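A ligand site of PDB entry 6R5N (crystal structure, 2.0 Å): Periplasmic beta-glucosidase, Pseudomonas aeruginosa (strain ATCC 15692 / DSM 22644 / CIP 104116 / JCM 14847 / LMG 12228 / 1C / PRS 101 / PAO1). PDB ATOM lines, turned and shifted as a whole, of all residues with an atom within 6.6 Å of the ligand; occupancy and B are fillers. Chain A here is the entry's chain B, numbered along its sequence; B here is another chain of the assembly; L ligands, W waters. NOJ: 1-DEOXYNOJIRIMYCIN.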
ATOM      1  N   PHE A  50       0.959 -34.898 -25.872  1.00  0.00           N
ATOM      2  CA  PHE A  50       0.131 -34.579 -24.685  1.00  0.00           C
ATOM      3  C   PHE A  50      -0.682 -35.823 -24.310  1.00  0.00           C
ATOM      4  O   PHE A  50      -0.841 -36.681 -25.174  1.00  0.00           O
ATOM      5  CB  PHE A  50      -0.683 -33.301 -24.882  1.00  0.00           C
ATOM      6  CG  PHE A  50      -1.776 -33.356 -25.924  1.00  0.00           C
ATOM      7  CD1 PHE A  50      -1.469 -33.397 -27.275  1.00  0.00           C
ATOM      8  CD2 PHE A  50      -3.105 -33.368 -25.530  1.00  0.00           C
ATOM      9  CE1 PHE A  50      -2.483 -33.448 -28.225  1.00  0.00           C
ATOM     10  CE2 PHE A  50      -4.117 -33.410 -26.484  1.00  0.00           C
ATOM     11  CZ  PHE A  50      -3.802 -33.450 -27.828  1.00  0.00           C
ATOM     12  N   ASN A  51      -1.046 -35.946 -23.027  1.00  0.00           N
ATOM     13  CA  ASN A  51      -1.899 -36.987 -22.382  1.00  0.00           C
ATOM     14  C   ASN A  51      -1.170 -38.319 -22.177  1.00  0.00           C
ATOM     15  O   ASN A  51      -1.844 -39.297 -21.788  1.00  0.00           O
ATOM     16  CB  ASN A  51      -3.203 -37.217 -23.135  1.00  0.00           C
ATOM     17  CG  ASN A  51      -4.138 -36.037 -23.015  1.00  0.00           C
ATOM     18  OD1 ASN A  51      -3.971 -35.205 -22.127  1.00  0.00           O
ATOM     19  ND2 ASN A  51      -5.064 -35.917 -23.947  1.00  0.00           N
ATOM     20  N   TYR A  78       0.541 -32.031 -20.431  1.00  0.00           N
ATOM     21  CA  TYR A  78      -0.703 -32.519 -19.796  1.00  0.00           C
ATOM     22  C   TYR A  78      -1.451 -31.338 -19.216  1.00  0.00           C
ATOM     23  O   TYR A  78      -0.882 -30.258 -19.049  1.00  0.00           O
ATOM     24  CB  TYR A  78      -0.344 -33.512 -18.691  1.00  0.00           C
ATOM     25  CG  TYR A  78      -1.456 -34.400 -18.211  1.00  0.00           C
ATOM     26  CD1 TYR A  78      -2.433 -34.892 -19.065  1.00  0.00           C
ATOM     27  CD2 TYR A  78      -1.489 -34.821 -16.882  1.00  0.00           C
ATOM     28  CE1 TYR A  78      -3.416 -35.758 -18.623  1.00  0.00           C
ATOM     29  CE2 TYR A  78      -2.455 -35.708 -16.426  1.00  0.00           C
ATOM     30  CZ  TYR A  78      -3.444 -36.157 -17.287  1.00  0.00           C
ATOM     31  OH  TYR A  78      -4.400 -36.997 -16.818  1.00  0.00           O
ATOM     32  N   ASP A  79      -2.729 -31.551 -18.928  1.00  0.00           N
ATOM     33  CA  ASP A  79      -3.620 -30.582 -18.274  1.00  0.00           C
ATOM     34  C   ASP A  79      -3.479 -30.760 -16.761  1.00  0.00           C
ATOM     35  O   ASP A  79      -4.352 -31.404 -16.140  1.00  0.00           O
ATOM     36  CB  ASP A  79      -5.035 -30.769 -18.796  1.00  0.00           C
ATOM     37  CG  ASP A  79      -5.153 -30.418 -20.265  1.00  0.00           C
ATOM     38  OD1 ASP A  79      -5.133 -29.211 -20.552  1.00  0.00           O
ATOM     39  OD2 ASP A  79      -5.225 -31.369 -21.125  1.00  0.00           O
ATOM     40  N   PHE A 123      -0.564 -27.420 -19.688  1.00  0.00           N
ATOM     41  CA  PHE A 123      -1.562 -26.516 -20.293  1.00  0.00           C
ATOM     42  C   PHE A 123      -2.294 -25.801 -19.150  1.00  0.00           C
ATOM     43  O   PHE A 123      -3.480 -26.058 -18.897  1.00  0.00           O
ATOM     44  CB  PHE A 123      -2.473 -27.308 -21.213  1.00  0.00           C
ATOM     45  CG  PHE A 123      -1.762 -28.021 -22.333  1.00  0.00           C
ATOM     46  CD1 PHE A 123      -0.673 -27.446 -22.974  1.00  0.00           C
ATOM     47  CD2 PHE A 123      -2.202 -29.254 -22.755  1.00  0.00           C
ATOM     48  CE1 PHE A 123      -0.052 -28.074 -24.036  1.00  0.00           C
ATOM     49  CE2 PHE A 123      -1.568 -29.886 -23.817  1.00  0.00           C
ATOM     50  CZ  PHE A 123      -0.492 -29.307 -24.458  1.00  0.00           C
ATOM     51  N   SER A 124      -1.551 -24.910 -18.516  1.00  0.00           N
ATOM     52  CA  SER A 124      -1.953 -24.169 -17.303  1.00  0.00           C
ATOM     53  C   SER A 124      -0.958 -23.027 -17.084  1.00  0.00           C
ATOM     54  O   SER A 124       0.176 -23.085 -17.585  1.00  0.00           O
ATOM     55  CB  SER A 124      -2.036 -25.121 -16.126  1.00  0.00           C
ATOM     56  OG  SER A 124      -2.410 -24.481 -14.902  1.00  0.00           O
ATOM     57  N   MET A 126      -4.943 -21.645 -16.561  1.00  0.00           N
ATOM     58  CA  MET A 126      -6.118 -21.062 -17.234  1.00  0.00           C
ATOM     59  C   MET A 126      -6.426 -19.740 -16.524  1.00  0.00           C
ATOM     60  O   MET A 126      -6.634 -19.757 -15.301  1.00  0.00           O
ATOM     61  CB  MET A 126      -7.309 -22.044 -17.159  1.00  0.00           C
ATOM     62  CG  MET A 126      -8.507 -21.606 -17.982  1.00  0.00           C
ATOM     63  SD  MET A 126      -9.523 -20.425 -17.057  1.00  0.00           S
ATOM     64  CE  MET A 126     -11.135 -20.700 -17.800  1.00  0.00           C
ATOM     65  N   ARG A 137     -16.526 -23.839 -17.826  1.00  0.00           N
ATOM     66  CA  ARG A 137     -15.068 -23.706 -17.550  1.00  0.00           C
ATOM     67  C   ARG A 137     -14.765 -22.613 -16.512  1.00  0.00           C
ATOM     68  O   ARG A 137     -13.586 -22.338 -16.291  1.00  0.00           O
ATOM     69  CB  ARG A 137     -14.347 -23.479 -18.859  1.00  0.00           C
ATOM     70  CG  ARG A 137     -14.718 -24.524 -19.902  1.00  0.00           C
ATOM     71  CD  ARG A 137     -13.750 -24.604 -21.060  1.00  0.00           C
ATOM     72  NE  ARG A 137     -12.469 -25.123 -20.595  1.00  0.00           N
ATOM     73  CZ  ARG A 137     -11.540 -25.644 -21.367  1.00  0.00           C
ATOM     74  NH1 ARG A 137     -11.715 -25.729 -22.668  1.00  0.00           N
ATOM     75  NH2 ARG A 137     -10.426 -26.059 -20.809  1.00  0.00           N
ATOM     76  N   GLU A 140     -12.246 -23.489 -13.780  1.00  0.00           N
ATOM     77  CA  GLU A 140     -10.793 -23.532 -14.124  1.00  0.00           C
ATOM     78  C   GLU A 140     -10.096 -22.174 -13.948  1.00  0.00           C
ATOM     79  O   GLU A 140      -8.853 -22.157 -13.986  1.00  0.00           O
ATOM     80  CB  GLU A 140     -10.609 -23.909 -15.585  1.00  0.00           C
ATOM     81  CG  GLU A 140     -11.096 -25.281 -15.880  1.00  0.00           C
ATOM     82  CD  GLU A 140     -11.222 -25.524 -17.377  1.00  0.00           C
ATOM     83  OE1 GLU A 140     -10.226 -25.277 -18.117  1.00  0.00           O
ATOM     84  OE2 GLU A 140     -12.325 -25.926 -17.783  1.00  0.00           O
ATOM     85  N   LYS A 176      -3.322 -20.269 -20.837  1.00  0.00           N
ATOM     86  CA  LYS A 176      -4.472 -20.438 -21.747  1.00  0.00           C
ATOM     87  C   LYS A 176      -5.629 -19.627 -21.159  1.00  0.00           C
ATOM     88  O   LYS A 176      -5.561 -19.251 -19.997  1.00  0.00           O
ATOM     89  CB  LYS A 176      -4.758 -21.938 -21.906  1.00  0.00           C
ATOM     90  CG  LYS A 176      -5.296 -22.650 -20.681  1.00  0.00           C
ATOM     91  CD  LYS A 176      -5.344 -24.152 -20.844  1.00  0.00           C
ATOM     92  CE  LYS A 176      -6.136 -24.886 -19.785  1.00  0.00           C
ATOM     93  NZ  LYS A 176      -6.002 -26.356 -19.985  1.00  0.00           N
ATOM     94  N   HIS A 177      -6.658 -19.338 -21.956  1.00  0.00           N
ATOM     95  CA  HIS A 177      -6.743 -19.586 -23.378  1.00  0.00           C
ATOM     96  C   HIS A 177      -6.712 -18.238 -24.089  1.00  0.00           C
ATOM     97  O   HIS A 177      -7.656 -17.446 -23.873  1.00  0.00           O
ATOM     98  CB  HIS A 177      -8.022 -20.321 -23.735  1.00  0.00           C
ATOM     99  CG  HIS A 177      -8.240 -21.598 -23.008  1.00  0.00           C
ATOM    100  ND1 HIS A 177      -8.796 -21.610 -21.752  1.00  0.00           N
ATOM    101  CD2 HIS A 177      -8.010 -22.878 -23.376  1.00  0.00           C
ATOM    102  CE1 HIS A 177      -8.927 -22.882 -21.384  1.00  0.00           C
ATOM    103  NE2 HIS A 177      -8.426 -23.680 -22.359  1.00  0.00           N
ATOM    104  N   TYR A 181     -11.743 -16.188 -23.975  1.00  0.00           N
ATOM    105  CA  TYR A 181     -12.505 -17.444 -24.123  1.00  0.00           C
ATOM    106  C   TYR A 181     -13.724 -17.472 -23.184  1.00  0.00           C
ATOM    107  O   TYR A 181     -14.814 -17.913 -23.599  1.00  0.00           O
ATOM    108  CB  TYR A 181     -11.511 -18.596 -23.942  1.00  0.00           C
ATOM    109  CG  TYR A 181     -12.063 -19.989 -24.092  1.00  0.00           C
ATOM    110  CD1 TYR A 181     -12.973 -20.321 -25.064  1.00  0.00           C
ATOM    111  CD2 TYR A 181     -11.603 -21.006 -23.268  1.00  0.00           C
ATOM    112  CE1 TYR A 181     -13.470 -21.623 -25.166  1.00  0.00           C
ATOM    113  CE2 TYR A 181     -12.063 -22.304 -23.366  1.00  0.00           C
ATOM    114  CZ  TYR A 181     -13.027 -22.615 -24.312  1.00  0.00           C
ATOM    115  OH  TYR A 181     -13.506 -23.897 -24.378  1.00  0.00           O
ATOM    116  N   TYR A 190     -17.294 -22.289 -26.541  1.00  0.00           N
ATOM    117  CA  TYR A 190     -16.734 -22.141 -27.903  1.00  0.00           C
ATOM    118  C   TYR A 190     -17.417 -20.971 -28.625  1.00  0.00           C
ATOM    119  O   TYR A 190     -17.015 -20.701 -29.803  1.00  0.00           O
ATOM    120  CB  TYR A 190     -16.928 -23.438 -28.682  1.00  0.00           C
ATOM    121  CG  TYR A 190     -16.520 -24.704 -27.980  1.00  0.00           C
ATOM    122  CD1 TYR A 190     -15.262 -24.862 -27.428  1.00  0.00           C
ATOM    123  CD2 TYR A 190     -17.416 -25.759 -27.860  1.00  0.00           C
ATOM    124  CE1 TYR A 190     -14.892 -26.042 -26.783  1.00  0.00           C
ATOM    125  CE2 TYR A 190     -17.061 -26.945 -27.241  1.00  0.00           C
ATOM    126  CZ  TYR A 190     -15.792 -27.088 -26.703  1.00  0.00           C
ATOM    127  OH  TYR A 190     -15.461 -28.285 -26.101  1.00  0.00           O
ATOM    128  N   MET A 220      -1.195 -20.981 -25.070  1.00  0.00           N
ATOM    129  CA  MET A 220      -2.201 -21.760 -25.832  1.00  0.00           C
ATOM    130  C   MET A 220      -3.259 -20.800 -26.378  1.00  0.00           C
ATOM    131  O   MET A 220      -3.878 -20.059 -25.579  1.00  0.00           O
ATOM    132  CB  MET A 220      -2.888 -22.824 -24.994  1.00  0.00           C
ATOM    133  CG  MET A 220      -3.861 -23.627 -25.862  1.00  0.00           C
ATOM    134  SD  MET A 220      -4.665 -24.982 -24.970  1.00  0.00           S
ATOM    135  CE  MET A 220      -3.292 -26.130 -24.871  1.00  0.00           C
ATOM    136  N   LEU A 223     -10.144 -21.126 -28.833  1.00  0.00           N
ATOM    137  CA  LEU A 223     -11.028 -21.704 -29.865  1.00  0.00           C
ATOM    138  C   LEU A 223     -12.065 -20.678 -30.368  1.00  0.00           C
ATOM    139  O   LEU A 223     -12.746 -20.992 -31.352  1.00  0.00           O
ATOM    140  CB  LEU A 223     -11.749 -22.911 -29.268  1.00  0.00           C
ATOM    141  CG  LEU A 223     -10.889 -24.135 -29.010  1.00  0.00           C
ATOM    142  CD1 LEU A 223     -11.647 -25.126 -28.163  1.00  0.00           C
ATOM    143  CD2 LEU A 223     -10.500 -24.783 -30.307  1.00  0.00           C
ATOM    144  N   ASP A 255      -5.142 -24.817 -29.790  1.00  0.00           N
ATOM    145  CA  ASP A 255      -6.016 -25.712 -28.992  1.00  0.00           C
ATOM    146  C   ASP A 255      -6.390 -26.889 -29.915  1.00  0.00           C
ATOM    147  O   ASP A 255      -5.956 -26.898 -31.097  1.00  0.00           O
ATOM    148  CB  ASP A 255      -7.182 -24.938 -28.361  1.00  0.00           C
ATOM    149  CG  ASP A 255      -7.806 -25.582 -27.124  1.00  0.00           C
ATOM    150  OD1 ASP A 255      -7.642 -26.815 -26.943  1.00  0.00           O
ATOM    151  OD2 ASP A 255      -8.493 -24.857 -26.353  1.00  0.00           O
ATOM    152  N   HIS A 256      -7.168 -27.837 -29.419  1.00  0.00           N
ATOM    153  CA  HIS A 256      -7.382 -29.150 -30.072  1.00  0.00           C
ATOM    154  C   HIS A 256      -8.215 -28.966 -31.346  1.00  0.00           C
ATOM    155  O   HIS A 256      -9.390 -28.575 -31.248  1.00  0.00           O
ATOM    156  CB  HIS A 256      -8.013 -30.105 -29.043  1.00  0.00           C
ATOM    157  CG  HIS A 256      -8.128 -31.515 -29.541  1.00  0.00           C
ATOM    158  ND1 HIS A 256      -8.976 -31.868 -30.593  1.00  0.00           N
ATOM    159  CD2 HIS A 256      -7.541 -32.650 -29.118  1.00  0.00           C
ATOM    160  CE1 HIS A 256      -8.877 -33.171 -30.803  1.00  0.00           C
ATOM    161  NE2 HIS A 256      -8.011 -33.661 -29.913  1.00  0.00           N
ATOM    162  N   MET A 287      -2.077 -28.691 -32.723  1.00  0.00           N
ATOM    163  CA  MET A 287      -2.597 -29.779 -31.842  1.00  0.00           C
ATOM    164  C   MET A 287      -3.605 -30.697 -32.570  1.00  0.00           C
ATOM    165  O   MET A 287      -4.682 -30.233 -32.998  1.00  0.00           O
ATOM    166  CB  MET A 287      -3.231 -29.196 -30.583  1.00  0.00           C
ATOM    167  CG  MET A 287      -3.584 -30.271 -29.559  1.00  0.00           C
ATOM    168  SD  MET A 287      -4.450 -29.673 -28.128  1.00  0.00           S
ATOM    169  CE  MET A 287      -3.147 -28.850 -27.234  1.00  0.00           C
ATOM    170  N   TRP A 398     -11.058 -31.598 -14.780  1.00  0.00           N
ATOM    171  CA  TRP A 398      -9.623 -31.459 -15.082  1.00  0.00           C
ATOM    172  C   TRP A 398      -8.808 -31.959 -13.886  1.00  0.00           C
ATOM    173  O   TRP A 398      -7.921 -31.219 -13.404  1.00  0.00           O
ATOM    174  CB  TRP A 398      -9.300 -30.005 -15.456  1.00  0.00           C
ATOM    175  CG  TRP A 398      -9.965 -29.588 -16.729  1.00  0.00           C
ATOM    176  CD1 TRP A 398     -11.015 -28.722 -16.862  1.00  0.00           C
ATOM    177  CD2 TRP A 398      -9.628 -30.017 -18.053  1.00  0.00           C
ATOM    178  NE1 TRP A 398     -11.325 -28.570 -18.191  1.00  0.00           N
ATOM    179  CE2 TRP A 398     -10.501 -29.361 -18.940  1.00  0.00           C
ATOM    180  CE3 TRP A 398      -8.668 -30.893 -18.586  1.00  0.00           C
ATOM    181  CZ2 TRP A 398     -10.441 -29.540 -20.319  1.00  0.00           C
ATOM    182  CZ3 TRP A 398      -8.602 -31.076 -19.942  1.00  0.00           C
ATOM    183  CH2 TRP A 398      -9.487 -30.408 -20.802  1.00  0.00           C
ATOM    184  N   GLU A 486     -15.501 -28.566 -19.468  1.00  0.00           N
ATOM    185  CA  GLU A 486     -15.493 -28.130 -20.891  1.00  0.00           C
ATOM    186  C   GLU A 486     -16.784 -28.619 -21.541  1.00  0.00           C
ATOM    187  O   GLU A 486     -17.123 -29.805 -21.370  1.00  0.00           O
ATOM    188  CB  GLU A 486     -14.284 -28.693 -21.664  1.00  0.00           C
ATOM    189  CG  GLU A 486     -14.308 -28.345 -23.145  1.00  0.00           C
ATOM    190  CD  GLU A 486     -13.132 -28.893 -23.929  1.00  0.00           C
ATOM    191  OE1 GLU A 486     -12.248 -29.521 -23.292  1.00  0.00           O
ATOM    192  OE2 GLU A 486     -13.110 -28.743 -25.202  1.00  0.00           O
ATOM    193  N   ARG B 585     -17.163 -25.182 -33.491  1.00  0.00           N
ATOM    194  CA  ARG B 585     -17.725 -26.463 -32.998  1.00  0.00           C
ATOM    195  C   ARG B 585     -19.243 -26.372 -32.898  1.00  0.00           C
ATOM    196  O   ARG B 585     -19.820 -26.495 -31.813  1.00  0.00           O
ATOM    197  CB  ARG B 585     -17.088 -26.837 -31.656  1.00  0.00           C
ATOM    198  CG  ARG B 585     -15.660 -27.332 -31.791  1.00  0.00           C
ATOM    199  CD  ARG B 585     -15.061 -27.548 -30.426  1.00  0.00           C
ATOM    200  NE  ARG B 585     -13.636 -27.823 -30.495  1.00  0.00           N
ATOM    201  CZ  ARG B 585     -12.971 -28.397 -29.513  1.00  0.00           C
ATOM    202  NH1 ARG B 585     -13.603 -28.764 -28.416  1.00  0.00           N
ATOM    203  NH2 ARG B 585     -11.669 -28.613 -29.647  1.00  0.00           N
HETATM  204  C1  NOJ L   1      -9.138 -28.610 -24.926  1.00  0.00           C
HETATM  205  C2  NOJ L   1      -9.116 -27.448 -23.933  1.00  0.00           C
HETATM  206  O2  NOJ L   1      -9.819 -26.392 -24.532  1.00  0.00           O
HETATM  207  C3  NOJ L   1      -7.751 -27.086 -23.318  1.00  0.00           C
HETATM  208  O3  NOJ L   1      -8.001 -26.437 -22.082  1.00  0.00           O
HETATM  209  C4  NOJ L   1      -6.813 -28.333 -23.228  1.00  0.00           C
HETATM  210  O4  NOJ L   1      -5.550 -27.892 -22.762  1.00  0.00           O
HETATM  211  C5  NOJ L   1      -6.671 -29.083 -24.574  1.00  0.00           C
HETATM  212  N5  NOJ L   1      -7.969 -29.407 -25.190  1.00  0.00           N
HETATM  213  C6  NOJ L   1      -5.913 -30.426 -24.471  1.00  0.00           C
HETATM  214  O6  NOJ L   1      -6.309 -31.267 -23.397  1.00  0.00           O
HETATM  215  O   HOH W   1      -7.151 -33.696 -23.901  1.00  0.00           O
HETATM  216  O   HOH W   2     -11.545 -30.196 -26.903  1.00  0.00           O
HETATM  217  O   HOH W   3     -10.238 -31.251 -24.235  1.00  0.00           O
HETATM  218  O   HOH W   4      -8.292 -31.949 -26.442  1.00  0.00           O
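O4 of the ligand sits close to SD of Met 220, at 3.8 Å. NE2 of His 177 sits at hydrogen-bond distance from O3 of the ligand (2.8 Å). OD2 of Asp 79 sits at hydrogen-bond distance from O6 of the ligand, at 2.5 Å. NH1 of Arg 137 is in hydrogen-bond range of O2 of the ligand (2.7 Å). The side-chain amino group (NZ) of Lys 176 lies within hydrogen-bond range of an oxygen (O3) of the ligand, 2.9 Å away. N5 of the ligand is in salt-bridge range of OD1 of Asp 255, 3.1 Å away.
The backbone NH (N) of Phe 123 lies within hydrogen-bond range of the backbone carbonyl oxygen (O) of Tyr 78 (2.9 Å). O of His 256 lies within hydrogen-bond range of NH2 of Arg 585 of chain B, at 2.8 Å. The guanidinium group (NH2) of Arg 137 is in salt-bridge range of the side-chain carboxylate (OE1) of Glu 140 (2.8 Å). O of Phe 123 lies within hydrogen-bond range of NZ of Lys 176 (2.8 Å). The side-chain carboxylate of Asp 79 lies within salt-bridge range of the side-chain amino group of Lys 176 (3.0 Å). OH of Tyr 181 sits at hydrogen-bond distance from NH1 of Arg 137 (3.1 Å). N of His 256 is in hydrogen-bond range of SD of Met 287, 3.5 Å away. OE2 of Glu 486 sits at hydrogen-bond distance from OH of Tyr 190 (2.6 Å).
Phe 123 touches the ligand (CB to O4, 3.5 Å). His 256 touches the ligand. Glu 486 touches the ligand (OE1 to C1, 3.6 Å). Hydrophobic or aromatic side chains that line the ligand: Phe 123, His 177, Met 220 and His 256. Within 4 Å of the ligand: Asp 79, Phe 123, Arg 137, Lys 176, His 177, Met 220, Asp 255, His 256 and Glu 486.
Water W1 lies within hydrogen-bond range of O6 of the ligand and ND2 of Asn 51. Water W3 lies within hydrogen-bond range of OE1 of Glu 486 (2.8 Å) and N5 of the ligand (3.1 Å). Water W2 bridges the side-chain carboxylate (OE2) of Glu 486 (2.7 Å) and the guanidinium group (NH1) of Arg 585 of chain B (2.9 Å).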
